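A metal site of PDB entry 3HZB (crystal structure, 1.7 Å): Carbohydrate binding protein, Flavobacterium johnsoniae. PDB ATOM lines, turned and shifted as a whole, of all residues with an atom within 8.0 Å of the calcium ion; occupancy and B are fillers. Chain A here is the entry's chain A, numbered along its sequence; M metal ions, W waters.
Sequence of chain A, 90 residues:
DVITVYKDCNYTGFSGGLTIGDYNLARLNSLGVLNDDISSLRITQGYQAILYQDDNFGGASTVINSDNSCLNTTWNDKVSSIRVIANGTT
The backbone carbonyl oxygen (O) of Gln 53 binds the calcium ion, at 2.4 Å. O of Lys 78 binds the calcium ion (2.5 Å). OD1 of Asp 36 binds the calcium ion. The calcium ion is bound by OG of Ser 80 (2.6 Å). The calcium ion is bound by water W1. The calcium ion is bound by water W3, 2.7 Å away. Water W2 binds the calcium ion. Slightly farther from the calcium ion lies water W4 (2.9 Å).
Water W4 lies within hydrogen-bond range of the side-chain amide oxygen (OD1) of Asn 35 (2.9 Å) and the side-chain carboxylate (OD2) of Asp 36 (3.2 Å).
Within 4 Å of the calcium ion: Asp 36, Gln 53, Lys 78 and Ser 80. The nearest printed residue that does not touch the calcium ion is Asn 35 (4.3 Å).
The side-chain amide nitrogen of Gln 53 lies within hydrogen-bond range of the backbone carbonyl oxygen of Thr 74, at 3.1 Å. The side-chain carboxylate (OD1) of Asp 36 sits close to the side-chain amide oxygen (OD1) of Asn 35 (3.4 Å). N of Asp 36 is in hydrogen-bond range of O of Val 79. The backbone NH (N) of Ser 80 sits at hydrogen-bond distance from the backbone carbonyl oxygen (O) of Tyr 52. The backbone NH of Leu 25 sits at hydrogen-bond distance from the backbone carbonyl oxygen of Ser 80.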
ATOM      1  N   LEU A  25      15.918 -24.419  26.535  1.00  0.00           N
ATOM      2  CA  LEU A  25      15.224 -23.211  26.969  1.00  0.00           C
ATOM      3  C   LEU A  25      14.008 -23.499  27.842  1.00  0.00           C
ATOM      4  O   LEU A  25      13.815 -22.870  28.885  1.00  0.00           O
ATOM      5  CB  LEU A  25      14.778 -22.383  25.766  1.00  0.00           C
ATOM      6  CG  LEU A  25      14.958 -20.858  25.854  1.00  0.00           C
ATOM      7  CD1 LEU A  25      13.961 -20.199  24.923  1.00  0.00           C
ATOM      8  CD2 LEU A  25      14.768 -20.365  27.278  1.00  0.00           C
ATOM      9  N   ASN A  35      15.725 -16.691  28.312  1.00  0.00           N
ATOM     10  CA  ASN A  35      16.596 -16.829  27.149  1.00  0.00           C
ATOM     11  C   ASN A  35      17.377 -15.528  26.988  1.00  0.00           C
ATOM     12  O   ASN A  35      16.877 -14.472  27.385  1.00  0.00           O
ATOM     13  CB  ASN A  35      15.739 -17.051  25.900  1.00  0.00           C
ATOM     14  CG  ASN A  35      16.564 -17.237  24.652  1.00  0.00           C
ATOM     15  OD1 ASN A  35      16.461 -16.453  23.703  1.00  0.00           O
ATOM     16  ND2 ASN A  35      17.381 -18.277  24.644  1.00  0.00           N
ATOM     17  N   ASP A  36      18.570 -15.602  26.405  1.00  0.00           N
ATOM     18  CA  ASP A  36      19.401 -14.423  26.173  1.00  0.00           C
ATOM     19  C   ASP A  36      19.305 -13.480  27.357  1.00  0.00           C
ATOM     20  O   ASP A  36      18.987 -12.304  27.201  1.00  0.00           O
ATOM     21  CB  ASP A  36      18.921 -13.684  24.910  1.00  0.00           C
ATOM     22  CG  ASP A  36      19.149 -14.499  23.647  1.00  0.00           C
ATOM     23  OD1 ASP A  36      19.723 -15.602  23.765  1.00  0.00           O
ATOM     24  OD2 ASP A  36      18.770 -14.040  22.556  1.00  0.00           O
ATOM     25  N   ASP A  37      19.622 -13.998  28.538  1.00  0.00           N
ATOM     26  CA  ASP A  37      19.492 -13.194  29.741  1.00  0.00           C
ATOM     27  C   ASP A  37      20.578 -13.432  30.794  1.00  0.00           C
ATOM     28  O   ASP A  37      20.842 -12.557  31.603  1.00  0.00           O
ATOM     29  CB  ASP A  37      18.115 -13.493  30.339  1.00  0.00           C
ATOM     30  CG  ASP A  37      17.714 -12.496  31.404  1.00  0.00           C
ATOM     31  OD1 ASP A  37      17.399 -12.946  32.522  1.00  0.00           O
ATOM     32  OD2 ASP A  37      17.705 -11.280  31.110  1.00  0.00           O
ATOM     33  N   TYR A  52      25.503 -22.736  25.277  1.00  0.00           N
ATOM     34  CA  TYR A  52      25.150 -22.816  23.859  1.00  0.00           C
ATOM     35  C   TYR A  52      24.424 -21.556  23.415  1.00  0.00           C
ATOM     36  O   TYR A  52      23.553 -21.058  24.120  1.00  0.00           O
ATOM     37  CB  TYR A  52      24.267 -24.021  23.609  1.00  0.00           C
ATOM     38  CG  TYR A  52      25.000 -25.326  23.775  1.00  0.00           C
ATOM     39  CD1 TYR A  52      25.722 -25.883  22.732  1.00  0.00           C
ATOM     40  CD2 TYR A  52      25.007 -25.972  25.011  1.00  0.00           C
ATOM     41  CE1 TYR A  52      26.444 -27.061  22.900  1.00  0.00           C
ATOM     42  CE2 TYR A  52      25.724 -27.150  25.193  1.00  0.00           C
ATOM     43  CZ  TYR A  52      26.443 -27.684  24.141  1.00  0.00           C
ATOM     44  OH  TYR A  52      27.163 -28.842  24.331  1.00  0.00           O
ATOM     45  N   GLN A  53      24.788 -21.061  22.233  1.00  0.00           N
ATOM     46  CA  GLN A  53      24.171 -19.862  21.696  1.00  0.00           C
ATOM     47  C   GLN A  53      22.696 -20.114  21.413  1.00  0.00           C
ATOM     48  O   GLN A  53      21.860 -19.294  21.742  1.00  0.00           O
ATOM     49  CB  GLN A  53      24.863 -19.414  20.406  1.00  0.00           C
ATOM     50  CG  GLN A  53      26.239 -18.795  20.602  1.00  0.00           C
ATOM     51  CD  GLN A  53      26.181 -17.394  21.183  1.00  0.00           C
ATOM     52  OE1 GLN A  53      25.353 -16.579  20.779  1.00  0.00           O
ATOM     53  NE2 GLN A  53      27.074 -17.110  22.127  1.00  0.00           N
ATOM     54  N   ASP A  54      22.377 -21.240  20.797  1.00  0.00           N
ATOM     55  CA  ASP A  54      20.994 -21.547  20.467  1.00  0.00           C
ATOM     56  C   ASP A  54      20.367 -22.590  21.377  1.00  0.00           C
ATOM     57  O   ASP A  54      21.057 -23.251  22.158  1.00  0.00           O
ATOM     58  CB  ASP A  54      20.892 -22.019  19.012  1.00  0.00           C
ATOM     59  CG  ASP A  54      21.589 -21.075  18.054  1.00  0.00           C
ATOM     60  OD1 ASP A  54      21.479 -19.848  18.252  1.00  0.00           O
ATOM     61  OD2 ASP A  54      22.219 -21.560  17.096  1.00  0.00           O
ATOM     62  N   ASP A  55      19.049 -22.728  21.283  1.00  0.00           N
ATOM     63  CA  ASP A  55      18.325 -23.697  22.094  1.00  0.00           C
ATOM     64  C   ASP A  55      18.666 -25.101  21.608  1.00  0.00           C
ATOM     65  O   ASP A  55      19.219 -25.286  20.519  1.00  0.00           O
ATOM     66  CB  ASP A  55      16.817 -23.437  21.969  1.00  0.00           C
ATOM     67  CG  ASP A  55      15.988 -24.263  22.950  1.00  0.00           C
ATOM     68  OD1 ASP A  55      16.563 -24.864  23.869  1.00  0.00           O
ATOM     69  OD2 ASP A  55      14.749 -24.290  22.788  1.00  0.00           O
ATOM     70  N   GLY A  58      22.444 -26.083  20.269  1.00  0.00           N
ATOM     71  CA  GLY A  58      22.895 -25.835  18.917  1.00  0.00           C
ATOM     72  C   GLY A  58      23.694 -24.542  18.876  1.00  0.00           C
ATOM     73  O   GLY A  58      23.696 -23.786  19.850  1.00  0.00           O
ATOM     74  N   THR A  74      30.225 -11.698  23.514  1.00  0.00           N
ATOM     75  CA  THR A  74      29.772 -12.827  22.702  1.00  0.00           C
ATOM     76  C   THR A  74      28.769 -13.701  23.442  1.00  0.00           C
ATOM     77  O   THR A  74      27.837 -14.239  22.848  1.00  0.00           O
ATOM     78  CB  THR A  74      30.947 -13.711  22.255  1.00  0.00           C
ATOM     79  OG1 THR A  74      31.784 -12.974  21.361  1.00  0.00           O
ATOM     80  CG2 THR A  74      30.436 -14.958  21.535  1.00  0.00           C
ATOM     81  N   TRP A  75      28.952 -13.827  24.758  1.00  0.00           N
ATOM     82  CA  TRP A  75      28.093 -14.683  25.569  1.00  0.00           C
ATOM     83  C   TRP A  75      27.095 -14.036  26.504  1.00  0.00           C
ATOM     84  O   TRP A  75      26.143 -14.692  26.928  1.00  0.00           O
ATOM     85  CB  TRP A  75      28.965 -15.678  26.332  1.00  0.00           C
ATOM     86  CG  TRP A  75      29.579 -16.671  25.403  1.00  0.00           C
ATOM     87  CD1 TRP A  75      30.809 -16.592  24.803  1.00  0.00           C
ATOM     88  CD2 TRP A  75      28.939 -17.831  24.875  1.00  0.00           C
ATOM     89  NE1 TRP A  75      30.962 -17.633  23.915  1.00  0.00           N
ATOM     90  CE2 TRP A  75      29.832 -18.409  23.944  1.00  0.00           C
ATOM     91  CE3 TRP A  75      27.696 -18.435  25.087  1.00  0.00           C
ATOM     92  CZ2 TRP A  75      29.520 -19.566  23.233  1.00  0.00           C
ATOM     93  CZ3 TRP A  75      27.382 -19.585  24.382  1.00  0.00           C
ATOM     94  CH2 TRP A  75      28.291 -20.138  23.458  1.00  0.00           C
ATOM     95  N   ASP A  77      23.938 -12.300  27.797  1.00  0.00           N
ATOM     96  CA  ASP A  77      22.573 -12.195  27.281  1.00  0.00           C
ATOM     97  C   ASP A  77      22.387 -12.913  25.955  1.00  0.00           C
ATOM     98  O   ASP A  77      21.655 -12.447  25.091  1.00  0.00           O
ATOM     99  CB  ASP A  77      22.177 -10.722  27.108  1.00  0.00           C
ATOM    100  CG  ASP A  77      22.120  -9.987  28.416  1.00  0.00           C
ATOM    101  OD1 ASP A  77      21.988 -10.684  29.432  1.00  0.00           O
ATOM    102  OD2 ASP A  77      22.197  -8.745  28.428  1.00  0.00           O
ATOM    103  N   LYS A  78      23.076 -14.040  25.792  1.00  0.00           N
ATOM    104  CA  LYS A  78      22.988 -14.804  24.550  1.00  0.00           C
ATOM    105  C   LYS A  78      22.757 -16.305  24.752  1.00  0.00           C
ATOM    106  O   LYS A  78      22.435 -17.016  23.806  1.00  0.00           O
ATOM    107  CB  LYS A  78      24.273 -14.619  23.743  1.00  0.00           C
ATOM    108  CG  LYS A  78      24.499 -13.207  23.236  1.00  0.00           C
ATOM    109  CD  LYS A  78      23.474 -12.830  22.182  1.00  0.00           C
ATOM    110  CE  LYS A  78      23.706 -11.426  21.654  1.00  0.00           C
ATOM    111  NZ  LYS A  78      22.656 -11.055  20.659  1.00  0.00           N
ATOM    112  N   VAL A  79      22.907 -16.795  25.983  1.00  0.00           N
ATOM    113  CA  VAL A  79      22.729 -18.219  26.243  1.00  0.00           C
ATOM    114  C   VAL A  79      21.286 -18.701  26.088  1.00  0.00           C
ATOM    115  O   VAL A  79      20.360 -18.095  26.612  1.00  0.00           O
ATOM    116  CB  VAL A  79      23.256 -18.580  27.649  1.00  0.00           C
ATOM    117  CG1 VAL A  79      22.953 -20.045  27.975  1.00  0.00           C
ATOM    118  CG2 VAL A  79      24.764 -18.324  27.710  1.00  0.00           C
ATOM    119  N   SER A  80      21.113 -19.803  25.370  1.00  0.00           N
ATOM    120  CA  SER A  80      19.784 -20.355  25.130  1.00  0.00           C
ATOM    121  C   SER A  80      19.573 -21.783  25.614  1.00  0.00           C
ATOM    122  O   SER A  80      18.447 -22.257  25.673  1.00  0.00           O
ATOM    123  CB  SER A  80      19.431 -20.264  23.658  1.00  0.00           C
ATOM    124  OG  SER A  80      19.237 -18.904  23.314  1.00  0.00           O
ATOM    125  N   SER A  81      20.664 -22.472  25.944  1.00  0.00           N
ATOM    126  CA  SER A  81      20.581 -23.830  26.461  1.00  0.00           C
ATOM    127  C   SER A  81      21.905 -24.128  27.115  1.00  0.00           C
ATOM    128  O   SER A  81      22.936 -23.534  26.759  1.00  0.00           O
ATOM    129  CB  SER A  81      20.271 -24.852  25.355  1.00  0.00           C
ATOM    130  OG  SER A  81      21.230 -24.840  24.324  1.00  0.00           O
HETATM  131 CA    CA M   1      20.661 -17.203  22.041  1.00  0.00          CA
HETATM  132  O   HOH W   1      19.835 -18.083  19.602  1.00  0.00           O
HETATM  133  O   HOH W   2      19.674 -15.113  20.374  1.00  0.00           O
HETATM  134  O   HOH W   3      22.526 -16.058  20.412  1.00  0.00           O
HETATM  135  O   HOH W   4      17.905 -16.832  21.187  1.00  0.00           O
